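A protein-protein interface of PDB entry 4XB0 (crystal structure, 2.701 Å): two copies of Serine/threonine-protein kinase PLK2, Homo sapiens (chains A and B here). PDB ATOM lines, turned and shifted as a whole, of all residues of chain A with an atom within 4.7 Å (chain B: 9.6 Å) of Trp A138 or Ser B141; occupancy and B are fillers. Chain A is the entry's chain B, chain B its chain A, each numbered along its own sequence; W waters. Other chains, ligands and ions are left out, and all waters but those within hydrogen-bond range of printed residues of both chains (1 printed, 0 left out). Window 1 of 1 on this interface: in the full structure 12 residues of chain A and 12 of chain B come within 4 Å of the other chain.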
ATOM      1  N   ASP A  42     -17.664   1.290  12.625  1.00  0.00           N
ATOM      2  CA  ASP A  42     -18.713   2.266  12.369  1.00  0.00           C
ATOM      3  C   ASP A  42     -19.689   2.405  13.537  1.00  0.00           C
ATOM      4  O   ASP A  42     -20.518   1.529  13.778  1.00  0.00           O
ATOM      5  CB  ASP A  42     -19.475   1.899  11.096  1.00  0.00           C
ATOM      6  CG  ASP A  42     -20.513   2.935  10.721  1.00  0.00           C
ATOM      7  OD1 ASP A  42     -20.403   4.090  11.183  1.00  0.00           O
ATOM      8  OD2 ASP A  42     -21.444   2.597   9.966  1.00  0.00           O
ATOM      9  N   SER A  44     -21.665   5.443  13.907  1.00  0.00           N
ATOM     10  CA  SER A  44     -21.983   6.784  13.424  1.00  0.00           C
ATOM     11  C   SER A  44     -23.156   7.444  14.142  1.00  0.00           C
ATOM     12  O   SER A  44     -23.262   8.669  14.155  1.00  0.00           O
ATOM     13  CB  SER A  44     -22.274   6.735  11.922  1.00  0.00           C
ATOM     14  OG  SER A  44     -21.170   6.221  11.200  1.00  0.00           O
ATOM     15  N   PHE A  49     -17.010   7.577  12.780  1.00  0.00           N
ATOM     16  CA  PHE A  49     -16.357   6.471  12.097  1.00  0.00           C
ATOM     17  C   PHE A  49     -14.899   6.388  12.526  1.00  0.00           C
ATOM     18  O   PHE A  49     -14.143   7.345  12.367  1.00  0.00           O
ATOM     19  CB  PHE A  49     -16.455   6.635  10.582  1.00  0.00           C
ATOM     20  CG  PHE A  49     -15.962   5.447   9.808  1.00  0.00           C
ATOM     21  CD1 PHE A  49     -14.653   5.392   9.360  1.00  0.00           C
ATOM     22  CD2 PHE A  49     -16.805   4.385   9.532  1.00  0.00           C
ATOM     23  CE1 PHE A  49     -14.194   4.303   8.648  1.00  0.00           C
ATOM     24  CE2 PHE A  49     -16.351   3.291   8.819  1.00  0.00           C
ATOM     25  CZ  PHE A  49     -15.043   3.251   8.378  1.00  0.00           C
ATOM     26  N   LEU A  61     -13.416  10.039  12.095  1.00  0.00           N
ATOM     27  CA  LEU A  61     -14.181  11.021  11.344  1.00  0.00           C
ATOM     28  C   LEU A  61     -15.527  11.206  12.018  1.00  0.00           C
ATOM     29  O   LEU A  61     -16.424  10.373  11.885  1.00  0.00           O
ATOM     30  CB  LEU A  61     -14.364  10.599   9.886  1.00  0.00           C
ATOM     31  CG  LEU A  61     -15.222  11.537   9.027  1.00  0.00           C
ATOM     32  CD1 LEU A  61     -14.847  12.996   9.246  1.00  0.00           C
ATOM     33  CD2 LEU A  61     -15.112  11.177   7.553  1.00  0.00           C
ATOM     34  N   LEU A 135      -9.215  10.486   6.951  1.00  0.00           N
ATOM     35  CA  LEU A 135     -10.392  10.163   6.162  1.00  0.00           C
ATOM     36  C   LEU A 135     -11.170  11.418   5.782  1.00  0.00           C
ATOM     37  O   LEU A 135     -11.617  12.168   6.650  1.00  0.00           O
ATOM     38  CB  LEU A 135     -11.292   9.203   6.939  1.00  0.00           C
ATOM     39  CG  LEU A 135     -12.442   8.561   6.171  1.00  0.00           C
ATOM     40  CD1 LEU A 135     -11.893   7.781   4.998  1.00  0.00           C
ATOM     41  CD2 LEU A 135     -13.253   7.662   7.085  1.00  0.00           C
ATOM     42  N   GLN A 137     -13.921  11.342   3.536  1.00  0.00           N
ATOM     43  CA  GLN A 137     -15.305  10.899   3.536  1.00  0.00           C
ATOM     44  C   GLN A 137     -15.371   9.397   3.308  1.00  0.00           C
ATOM     45  O   GLN A 137     -14.425   8.793   2.804  1.00  0.00           O
ATOM     46  CB  GLN A 137     -16.110  11.645   2.468  1.00  0.00           C
ATOM     47  CG  GLN A 137     -15.555  11.521   1.062  1.00  0.00           C
ATOM     48  CD  GLN A 137     -16.422  12.219   0.033  1.00  0.00           C
ATOM     49  OE1 GLN A 137     -17.649  12.216   0.134  1.00  0.00           O
ATOM     50  NE2 GLN A 137     -15.787  12.831  -0.960  1.00  0.00           N
ATOM     51  N   TRP A 138     -16.497   8.797   3.672  1.00  0.00           N
ATOM     52  CA  TRP A 138     -16.694   7.370   3.471  1.00  0.00           C
ATOM     53  C   TRP A 138     -18.133   7.074   3.082  1.00  0.00           C
ATOM     54  O   TRP A 138     -19.032   7.874   3.336  1.00  0.00           O
ATOM     55  CB  TRP A 138     -16.296   6.586   4.724  1.00  0.00           C
ATOM     56  CG  TRP A 138     -17.084   6.931   5.943  1.00  0.00           C
ATOM     57  CD1 TRP A 138     -16.783   7.891   6.862  1.00  0.00           C
ATOM     58  CD2 TRP A 138     -18.291   6.306   6.393  1.00  0.00           C
ATOM     59  NE1 TRP A 138     -17.733   7.912   7.852  1.00  0.00           N
ATOM     60  CE2 TRP A 138     -18.670   6.947   7.588  1.00  0.00           C
ATOM     61  CE3 TRP A 138     -19.091   5.271   5.901  1.00  0.00           C
ATOM     62  CZ2 TRP A 138     -19.812   6.588   8.298  1.00  0.00           C
ATOM     63  CZ3 TRP A 138     -20.226   4.916   6.607  1.00  0.00           C
ATOM     64  CH2 TRP A 138     -20.575   5.573   7.792  1.00  0.00           C
ATOM     65  N   LEU A 139     -18.348   5.921   2.462  1.00  0.00           N
ATOM     66  CA  LEU A 139     -19.698   5.493   2.142  1.00  0.00           C
ATOM     67  C   LEU A 139     -19.824   3.981   2.231  1.00  0.00           C
ATOM     68  O   LEU A 139     -18.904   3.244   1.878  1.00  0.00           O
ATOM     69  CB  LEU A 139     -20.075   5.975   0.738  1.00  0.00           C
ATOM     70  CG  LEU A 139     -21.535   5.904   0.292  1.00  0.00           C
ATOM     71  CD1 LEU A 139     -22.182   7.269   0.426  1.00  0.00           C
ATOM     72  CD2 LEU A 139     -21.637   5.404  -1.139  1.00  0.00           C
ATOM     73  N   LYS A 140     -20.979   3.526   2.700  1.00  0.00           N
ATOM     74  CA  LYS A 140     -21.211   2.107   2.913  1.00  0.00           C
ATOM     75  C   LYS A 140     -22.462   1.674   2.178  1.00  0.00           C
ATOM     76  O   LYS A 140     -23.486   2.341   2.253  1.00  0.00           O
ATOM     77  CB  LYS A 140     -21.358   1.788   4.403  1.00  0.00           C
ATOM     78  CG  LYS A 140     -20.080   1.349   5.089  1.00  0.00           C
ATOM     79  CD  LYS A 140     -20.354   0.317   6.173  1.00  0.00           C
ATOM     80  CE  LYS A 140     -21.111   0.901   7.347  1.00  0.00           C
ATOM     81  NZ  LYS A 140     -21.448  -0.146   8.351  1.00  0.00           N
ATOM     82  N   LEU A 145     -17.710  -1.085   1.791  1.00  0.00           N
ATOM     83  CA  LEU A 145     -17.356   0.169   2.442  1.00  0.00           C
ATOM     84  C   LEU A 145     -16.302   0.879   1.613  1.00  0.00           C
ATOM     85  O   LEU A 145     -15.277   0.297   1.266  1.00  0.00           O
ATOM     86  CB  LEU A 145     -16.837  -0.058   3.862  1.00  0.00           C
ATOM     87  CG  LEU A 145     -15.953   1.070   4.410  1.00  0.00           C
ATOM     88  CD1 LEU A 145     -16.748   2.336   4.700  1.00  0.00           C
ATOM     89  CD2 LEU A 145     -15.202   0.621   5.647  1.00  0.00           C
ATOM     90  N   MET A 146     -16.555   2.142   1.299  1.00  0.00           N
ATOM     91  CA  MET A 146     -15.631   2.911   0.488  1.00  0.00           C
ATOM     92  C   MET A 146     -15.067   4.062   1.303  1.00  0.00           C
ATOM     93  O   MET A 146     -15.814   4.814   1.921  1.00  0.00           O
ATOM     94  CB  MET A 146     -16.327   3.437  -0.767  1.00  0.00           C
ATOM     95  CG  MET A 146     -15.416   4.194  -1.714  1.00  0.00           C
ATOM     96  SD  MET A 146     -15.334   5.969  -1.394  1.00  0.00           S
ATOM     97  CE  MET A 146     -16.938   6.497  -1.985  1.00  0.00           C
ATOM     98  N   MET A 147     -13.747   4.195   1.303  1.00  0.00           N
ATOM     99  CA  MET A 147     -13.102   5.285   2.019  1.00  0.00           C
ATOM    100  C   MET A 147     -12.156   6.060   1.114  1.00  0.00           C
ATOM    101  O   MET A 147     -11.369   5.477   0.369  1.00  0.00           O
ATOM    102  CB  MET A 147     -12.337   4.770   3.242  1.00  0.00           C
ATOM    103  CG  MET A 147     -13.113   3.825   4.140  1.00  0.00           C
ATOM    104  SD  MET A 147     -12.092   3.212   5.495  1.00  0.00           S
ATOM    105  CE  MET A 147     -11.702   1.563   4.925  1.00  0.00           C
ATOM    106  N   TRP B  40     -33.409   0.978  13.887  1.00  0.00           N
ATOM    107  CA  TRP B  40     -32.500   0.357  12.929  1.00  0.00           C
ATOM    108  C   TRP B  40     -31.213  -0.113  13.587  1.00  0.00           C
ATOM    109  O   TRP B  40     -30.805   0.416  14.614  1.00  0.00           O
ATOM    110  CB  TRP B  40     -32.175   1.327  11.792  1.00  0.00           C
ATOM    111  CG  TRP B  40     -31.423   2.551  12.216  1.00  0.00           C
ATOM    112  CD1 TRP B  40     -31.957   3.731  12.652  1.00  0.00           C
ATOM    113  CD2 TRP B  40     -30.013   2.741  12.208  1.00  0.00           C
ATOM    114  NE1 TRP B  40     -30.964   4.632  12.936  1.00  0.00           N
ATOM    115  CE2 TRP B  40     -29.730   4.036  12.662  1.00  0.00           C
ATOM    116  CE3 TRP B  40     -28.919   1.921  11.857  1.00  0.00           C
ATOM    117  CZ2 TRP B  40     -28.457   4.558  12.788  1.00  0.00           C
ATOM    118  CZ3 TRP B  40     -27.641   2.429  11.978  1.00  0.00           C
ATOM    119  CH2 TRP B  40     -27.420   3.732  12.439  1.00  0.00           C
ATOM    120  N   ASP B  42     -27.217  -1.518  12.356  1.00  0.00           N
ATOM    121  CA  ASP B  42     -26.252  -1.842  11.315  1.00  0.00           C
ATOM    122  C   ASP B  42     -25.182  -2.792  11.835  1.00  0.00           C
ATOM    123  O   ASP B  42     -24.293  -2.394  12.589  1.00  0.00           O
ATOM    124  CB  ASP B  42     -25.582  -0.583  10.768  1.00  0.00           C
ATOM    125  CG  ASP B  42     -24.631  -0.888   9.628  1.00  0.00           C
ATOM    126  OD1 ASP B  42     -24.781  -1.957   9.000  1.00  0.00           O
ATOM    127  OD2 ASP B  42     -23.713  -0.084   9.376  1.00  0.00           O
ATOM    128  N   SER B  44     -23.393  -4.849   9.500  1.00  0.00           N
ATOM    129  CA  SER B  44     -23.144  -5.299   8.137  1.00  0.00           C
ATOM    130  C   SER B  44     -21.816  -6.032   8.021  1.00  0.00           C
ATOM    131  O   SER B  44     -21.596  -6.783   7.075  1.00  0.00           O
ATOM    132  CB  SER B  44     -23.181  -4.115   7.165  1.00  0.00           C
ATOM    133  OG  SER B  44     -22.649  -2.944   7.752  1.00  0.00           O
ATOM    134  N   TRP B 138     -29.922  -0.010   0.940  1.00  0.00           N
ATOM    135  CA  TRP B 138     -29.594   1.055   1.876  1.00  0.00           C
ATOM    136  C   TRP B 138     -28.155   1.485   1.636  1.00  0.00           C
ATOM    137  O   TRP B 138     -27.353   0.707   1.123  1.00  0.00           O
ATOM    138  CB  TRP B 138     -29.767   0.586   3.321  1.00  0.00           C
ATOM    139  CG  TRP B 138     -28.834  -0.530   3.695  1.00  0.00           C
ATOM    140  CD1 TRP B 138     -29.061  -1.868   3.567  1.00  0.00           C
ATOM    141  CD2 TRP B 138     -27.529  -0.400   4.271  1.00  0.00           C
ATOM    142  NE1 TRP B 138     -27.976  -2.580   4.018  1.00  0.00           N
ATOM    143  CE2 TRP B 138     -27.019  -1.698   4.458  1.00  0.00           C
ATOM    144  CE3 TRP B 138     -26.737   0.692   4.645  1.00  0.00           C
ATOM    145  CZ2 TRP B 138     -25.760  -1.939   5.000  1.00  0.00           C
ATOM    146  CZ3 TRP B 138     -25.485   0.453   5.183  1.00  0.00           C
ATOM    147  CH2 TRP B 138     -25.010  -0.852   5.356  1.00  0.00           C
ATOM    148  N   LEU B 139     -27.822   2.717   2.003  1.00  0.00           N
ATOM    149  CA  LEU B 139     -26.428   3.138   1.989  1.00  0.00           C
ATOM    150  C   LEU B 139     -26.173   4.202   3.050  1.00  0.00           C
ATOM    151  O   LEU B 139     -27.047   5.011   3.358  1.00  0.00           O
ATOM    152  CB  LEU B 139     -26.000   3.624   0.597  1.00  0.00           C
ATOM    153  CG  LEU B 139     -26.571   4.862  -0.091  1.00  0.00           C
ATOM    154  CD1 LEU B 139     -25.830   6.123   0.321  1.00  0.00           C
ATOM    155  CD2 LEU B 139     -26.503   4.677  -1.600  1.00  0.00           C
ATOM    156  N   LYS B 140     -24.966   4.191   3.605  1.00  0.00           N
ATOM    157  CA  LYS B 140     -24.621   5.073   4.710  1.00  0.00           C
ATOM    158  C   LYS B 140     -23.411   5.935   4.391  1.00  0.00           C
ATOM    159  O   LYS B 140     -22.416   5.453   3.852  1.00  0.00           O
ATOM    160  CB  LYS B 140     -24.342   4.264   5.974  1.00  0.00           C
ATOM    161  CG  LYS B 140     -25.533   4.108   6.892  1.00  0.00           C
ATOM    162  CD  LYS B 140     -25.092   4.082   8.340  1.00  0.00           C
ATOM    163  CE  LYS B 140     -24.306   2.830   8.641  1.00  0.00           C
ATOM    164  NZ  LYS B 140     -23.778   2.818  10.033  1.00  0.00           N
ATOM    165  N   SER B 141     -23.507   7.215   4.729  1.00  0.00           N
ATOM    166  CA  SER B 141     -22.368   8.116   4.646  1.00  0.00           C
ATOM    167  C   SER B 141     -21.971   8.547   6.051  1.00  0.00           C
ATOM    168  O   SER B 141     -22.505   8.040   7.037  1.00  0.00           O
ATOM    169  CB  SER B 141     -22.691   9.334   3.782  1.00  0.00           C
ATOM    170  OG  SER B 141     -23.687  10.138   4.387  1.00  0.00           O
ATOM    171  N   ASP B 142     -21.023   9.473   6.140  1.00  0.00           N
ATOM    172  CA  ASP B 142     -20.574   9.984   7.429  1.00  0.00           C
ATOM    173  C   ASP B 142     -21.608  10.898   8.081  1.00  0.00           C
ATOM    174  O   ASP B 142     -21.476  11.261   9.249  1.00  0.00           O
ATOM    175  CB  ASP B 142     -19.250  10.731   7.263  1.00  0.00           C
ATOM    176  CG  ASP B 142     -19.252  11.663   6.069  1.00  0.00           C
ATOM    177  OD1 ASP B 142     -19.165  11.164   4.926  1.00  0.00           O
ATOM    178  OD2 ASP B 142     -19.341  12.892   6.274  1.00  0.00           O
ATOM    179  N   LYS B 143     -22.639  11.264   7.325  1.00  0.00           N
ATOM    180  CA  LYS B 143     -23.641  12.200   7.818  1.00  0.00           C
ATOM    181  C   LYS B 143     -25.032  11.600   8.018  1.00  0.00           C
ATOM    182  O   LYS B 143     -25.767  12.029   8.906  1.00  0.00           O
ATOM    183  CB  LYS B 143     -23.747  13.392   6.865  1.00  0.00           C
ATOM    184  CG  LYS B 143     -22.445  14.142   6.649  1.00  0.00           C
ATOM    185  CD  LYS B 143     -22.433  15.445   7.428  1.00  0.00           C
ATOM    186  CE  LYS B 143     -21.060  16.092   7.420  1.00  0.00           C
ATOM    187  NZ  LYS B 143     -21.070  17.408   8.118  1.00  0.00           N
ATOM    188  N   ALA B 144     -25.397  10.610   7.209  1.00  0.00           N
ATOM    189  CA  ALA B 144     -26.770  10.114   7.236  1.00  0.00           C
ATOM    190  C   ALA B 144     -26.927   8.656   6.814  1.00  0.00           C
ATOM    191  O   ALA B 144     -26.058   8.085   6.157  1.00  0.00           O
ATOM    192  CB  ALA B 144     -27.648  10.996   6.358  1.00  0.00           C
ATOM    193  N   LEU B 145     -28.056   8.071   7.203  1.00  0.00           N
ATOM    194  CA  LEU B 145     -28.439   6.726   6.785  1.00  0.00           C
ATOM    195  C   LEU B 145     -29.629   6.799   5.841  1.00  0.00           C
ATOM    196  O   LEU B 145     -30.652   7.395   6.171  1.00  0.00           O
ATOM    197  CB  LEU B 145     -28.783   5.860   7.998  1.00  0.00           C
ATOM    198  CG  LEU B 145     -29.698   4.651   7.771  1.00  0.00           C
ATOM    199  CD1 LEU B 145     -29.014   3.543   6.989  1.00  0.00           C
ATOM    200  CD2 LEU B 145     -30.204   4.129   9.102  1.00  0.00           C
ATOM    201  N   MET B 146     -29.501   6.183   4.671  1.00  0.00           N
ATOM    202  CA  MET B 146     -30.565   6.227   3.676  1.00  0.00           C
ATOM    203  C   MET B 146     -31.121   4.835   3.385  1.00  0.00           C
ATOM    204  O   MET B 146     -30.368   3.904   3.106  1.00  0.00           O
ATOM    205  CB  MET B 146     -30.053   6.876   2.388  1.00  0.00           C
ATOM    206  CG  MET B 146     -31.120   7.046   1.330  1.00  0.00           C
ATOM    207  SD  MET B 146     -31.276   5.685   0.158  1.00  0.00           S
ATOM    208  CE  MET B 146     -29.840   5.957  -0.868  1.00  0.00           C
ATOM    209  N   MET B 147     -32.442   4.699   3.447  1.00  0.00           N
ATOM    210  CA  MET B 147     -33.099   3.426   3.164  1.00  0.00           C
ATOM    211  C   MET B 147     -34.219   3.575   2.137  1.00  0.00           C
ATOM    212  O   MET B 147     -35.043   4.482   2.237  1.00  0.00           O
ATOM    213  CB  MET B 147     -33.661   2.828   4.456  1.00  0.00           C
ATOM    214  CG  MET B 147     -32.684   2.830   5.615  1.00  0.00           C
ATOM    215  SD  MET B 147     -33.431   2.258   7.149  1.00  0.00           S
ATOM    216  CE  MET B 147     -33.666   3.810   8.010  1.00  0.00           C
ATOM    217  N   VAL B 156     -34.453   8.868   5.259  1.00  0.00           N
ATOM    218  CA  VAL B 156     -33.087   9.256   5.587  1.00  0.00           C
ATOM    219  C   VAL B 156     -32.960   9.683   7.047  1.00  0.00           C
ATOM    220  O   VAL B 156     -33.609  10.632   7.483  1.00  0.00           O
ATOM    221  CB  VAL B 156     -32.593  10.397   4.680  1.00  0.00           C
ATOM    222  CG1 VAL B 156     -31.211  10.856   5.113  1.00  0.00           C
ATOM    223  CG2 VAL B 156     -32.573   9.945   3.231  1.00  0.00           C
ATOM    224  N   ASN B 157     -32.120   8.976   7.795  1.00  0.00           N
ATOM    225  CA  ASN B 157     -31.847   9.325   9.184  1.00  0.00           C
ATOM    226  C   ASN B 157     -30.523  10.063   9.333  1.00  0.00           C
ATOM    227  O   ASN B 157     -29.504   9.636   8.795  1.00  0.00           O
ATOM    228  CB  ASN B 157     -31.837   8.070  10.061  1.00  0.00           C
ATOM    229  CG  ASN B 157     -33.194   7.407  10.150  1.00  0.00           C
ATOM    230  OD1 ASN B 157     -34.025   7.544   9.253  1.00  0.00           O
ATOM    231  ND2 ASN B 157     -33.425   6.678  11.234  1.00  0.00           N
ATOM    232  N   PHE B 158     -30.545  11.172  10.066  1.00  0.00           N
ATOM    233  CA  PHE B 158     -29.326  11.908  10.381  1.00  0.00           C
ATOM    234  C   PHE B 158     -28.873  11.586  11.802  1.00  0.00           C
ATOM    235  O   PHE B 158     -29.697  11.396  12.694  1.00  0.00           O
ATOM    236  CB  PHE B 158     -29.545  13.411  10.203  1.00  0.00           C
ATOM    237  CG  PHE B 158     -29.960  13.796   8.813  1.00  0.00           C
ATOM    238  CD1 PHE B 158     -31.295  13.778   8.444  1.00  0.00           C
ATOM    239  CD2 PHE B 158     -29.016  14.170   7.871  1.00  0.00           C
ATOM    240  CE1 PHE B 158     -31.680  14.125   7.164  1.00  0.00           C
ATOM    241  CE2 PHE B 158     -29.395  14.522   6.591  1.00  0.00           C
ATOM    242  CZ  PHE B 158     -30.728  14.499   6.237  1.00  0.00           C
ATOM    243  N   TYR B 159     -27.562  11.527  12.008  1.00  0.00           N
ATOM    244  CA  TYR B 159     -27.013  11.041  13.271  1.00  0.00           C
ATOM    245  C   TYR B 159     -27.072  12.054  14.417  1.00  0.00           C
ATOM    246  O   TYR B 159     -27.684  11.789  15.446  1.00  0.00           O
ATOM    247  CB  TYR B 159     -25.564  10.589  13.070  1.00  0.00           C
ATOM    248  CG  TYR B 159     -25.355   9.671  11.885  1.00  0.00           C
ATOM    249  CD1 TYR B 159     -26.220   8.612  11.635  1.00  0.00           C
ATOM    250  CD2 TYR B 159     -24.285   9.859  11.020  1.00  0.00           C
ATOM    251  CE1 TYR B 159     -26.028   7.771  10.556  1.00  0.00           C
ATOM    252  CE2 TYR B 159     -24.086   9.023   9.939  1.00  0.00           C
ATOM    253  CZ  TYR B 159     -24.959   7.982   9.712  1.00  0.00           C
ATOM    254  OH  TYR B 159     -24.761   7.154   8.637  1.00  0.00           O
ATOM    255  N   TYR B 208     -29.731  17.073   1.065  1.00  0.00           N
ATOM    256  CA  TYR B 208     -28.768  16.022   1.365  1.00  0.00           C
ATOM    257  C   TYR B 208     -29.329  14.638   1.073  1.00  0.00           C
ATOM    258  O   TYR B 208     -28.616  13.760   0.587  1.00  0.00           O
ATOM    259  CB  TYR B 208     -28.313  16.101   2.821  1.00  0.00           C
ATOM    260  CG  TYR B 208     -27.092  15.256   3.083  1.00  0.00           C
ATOM    261  CD1 TYR B 208     -25.831  15.695   2.701  1.00  0.00           C
ATOM    262  CD2 TYR B 208     -27.199  14.013   3.692  1.00  0.00           C
ATOM    263  CE1 TYR B 208     -24.710  14.924   2.927  1.00  0.00           C
ATOM    264  CE2 TYR B 208     -26.081  13.235   3.922  1.00  0.00           C
ATOM    265  CZ  TYR B 208     -24.840  13.697   3.538  1.00  0.00           C
ATOM    266  OH  TYR B 208     -23.722  12.927   3.763  1.00  0.00           O
ATOM    267  N   ALA B 209     -30.605  14.446   1.391  1.00  0.00           N
ATOM    268  CA  ALA B 209     -31.282  13.181   1.140  1.00  0.00           C
ATOM    269  C   ALA B 209     -31.241  12.857  -0.347  1.00  0.00           C
ATOM    270  O   ALA B 209     -31.132  11.696  -0.742  1.00  0.00           O
ATOM    271  CB  ALA B 209     -32.716  13.235   1.638  1.00  0.00           C
ATOM    272  N   ASN B 211     -28.885  13.903  -2.538  1.00  0.00           N
ATOM    273  CA  ASN B 211     -27.520  13.561  -2.924  1.00  0.00           C
ATOM    274  C   ASN B 211     -27.209  12.102  -2.620  1.00  0.00           C
ATOM    275  O   ASN B 211     -26.349  11.491  -3.255  1.00  0.00           O
ATOM    276  CB  ASN B 211     -26.511  14.461  -2.211  1.00  0.00           C
ATOM    277  CG  ASN B 211     -26.254  15.754  -2.957  1.00  0.00           C
ATOM    278  OD1 ASN B 211     -26.445  15.834  -4.169  1.00  0.00           O
ATOM    279  ND2 ASN B 211     -25.806  16.774  -2.234  1.00  0.00           N
ATOM    280  N   MET B 212     -27.925  11.550  -1.647  1.00  0.00           N
ATOM    281  CA  MET B 212     -27.722  10.172  -1.228  1.00  0.00           C
ATOM    282  C   MET B 212     -28.407   9.235  -2.209  1.00  0.00           C
ATOM    283  O   MET B 212     -27.956   8.113  -2.439  1.00  0.00           O
ATOM    284  CB  MET B 212     -28.263   9.957   0.184  1.00  0.00           C
ATOM    285  CG  MET B 212     -27.418  10.598   1.270  1.00  0.00           C
ATOM    286  SD  MET B 212     -27.612   9.807   2.876  1.00  0.00           S
ATOM    287  CE  MET B 212     -26.195   8.715   2.886  1.00  0.00           C
ATOM    288  N   LEU B 213     -29.502   9.711  -2.792  1.00  0.00           N
ATOM    289  CA  LEU B 213     -30.250   8.938  -3.772  1.00  0.00           C
ATOM    290  C   LEU B 213     -29.482   8.887  -5.089  1.00  0.00           C
ATOM    291  O   LEU B 213     -29.419   7.848  -5.747  1.00  0.00           O
ATOM    292  CB  LEU B 213     -31.642   9.539  -3.974  1.00  0.00           C
ATOM    293  CG  LEU B 213     -32.783   8.576  -4.295  1.00  0.00           C
ATOM    294  CD1 LEU B 213     -32.640   7.291  -3.494  1.00  0.00           C
ATOM    295  CD2 LEU B 213     -34.122   9.234  -4.007  1.00  0.00           C
HETATM  296  O   HOH W   1     -19.920  12.021   2.031  1.00  0.00           O
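The side-chain amino group (NZ) of Lys A140 lies within salt-bridge range of the side-chain carboxylate (OD2) of Asp B42, at 2.5 Å.
OG of Ser B44 is in hydrogen-bond range of NZ of Lys A140 (3.1 Å).
The side-chain amino group (NZ) of Lys B140 is in salt-bridge range of the side-chain carboxylate (OD1) of Asp A42, at 3.8 Å.
O of Lys B140 lies within hydrogen-bond range of N of Lys A140 (2.7 Å).
The side-chain carboxylate (OD2) of Asp B42 lies within salt-bridge range of the side-chain amino group (NZ) of Lys B140 (3.0 Å).
O of Met B146 sits at hydrogen-bond distance from N of Leu B139.
The backbone carbonyl oxygen (O) of Ser B141 lies within hydrogen-bond range of the side-chain hydroxyl (OH) of Tyr B159, at 2.9 Å.
The side-chain carboxylate of Asp A42 sits at hydrogen-bond distance from the backbone NH of Ser A44, 3.3 Å away.
The side-chain carboxylate of Asp A42 lies within salt-bridge range of the side-chain amino group of Lys A140 (3.2 Å).
The backbone carbonyl oxygen (O) of Leu A139 is in hydrogen-bond range of the backbone NH (N) of Met A146 (2.7 Å).
Asp A42 touches Asp B42 (OD2 to OD2, 3.6 Å).
CB of Tyr B159 touches O of Ser A44, at 3.2 Å.
Asp B142 touches Gln A137.
Trp A138 touches Lys B140 (CZ3 to O, 3.6 Å).
CH2 of Trp A138 touches O of Ser B141, 3.2 Å away.
Trp A138 touches Asp B142.
Leu A139 touches Leu B139.
Lys B140 touches Leu A139 (O to CA, 3.2 Å).
Leu A139 touches Ser B141.
Leu B139 touches Lys A140.
Of chain B, only Lys B140, Ser B141 and Asp B142 come within 4 Å of Trp A138.
Of the printed residues of chain B, Leu A139 touches Leu B139 (3.8 Å), Lys B140 (3.2 Å) and Ser B141 (3.97 Å).
Printed residues of chain A within 4 Å of Leu B139: Leu A139 (3.8 Å) and Lys A140 (3.1 Å).
Of chain A, only Trp A138 (3.2 Å) and Leu A139 (3.97 Å) come within 4 Å of Ser B141.
Lys B143 touches none of the printed residues of chain A.
Tyr B208 touches none of the printed residues of chain A.
The nearest printed residue of chain A that does not touch Ser B141 is Ser A44 (4.7 Å).
Hydrophobic or aromatic side chains of chain A within 4 Å of the printed part of chain B: Trp A138 and Leu A139.
Of the 22 printed residues of chain B, 7 touch a printed residue of chain A.
Among the printed residues, 14 pairs touch across the chains.
Among the printed residues, Asp or Glu carboxylates within 4 Å of a Lys or Arg side-chain nitrogen of the other chain: Asp A42 with Lys B140 (2.3 Å) and Lys A140 with Asp B42 (2.5 Å).
Trp A138 touches Lys B140, but with the chains exchanged Lys A140 does not touch Trp B138 (4.02 Å).
Leu A139 touches its own counterpart, Leu B139.
Leu A139 touches Lys B140, and with the chains exchanged Lys A140 touches Leu B139.
Lys B140 touches its own counterpart, Lys A140.
8 positions are printed for both chains.
Of the 14 pairs that touch across the chains among the printed residues, 7 have their exchanged pair printed and touching as well.
Water W1 bridges the side-chain amide oxygen of Gln A137 (3.0 Å) and the side-chain carboxylate of Asp B142 (3.1 Å).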
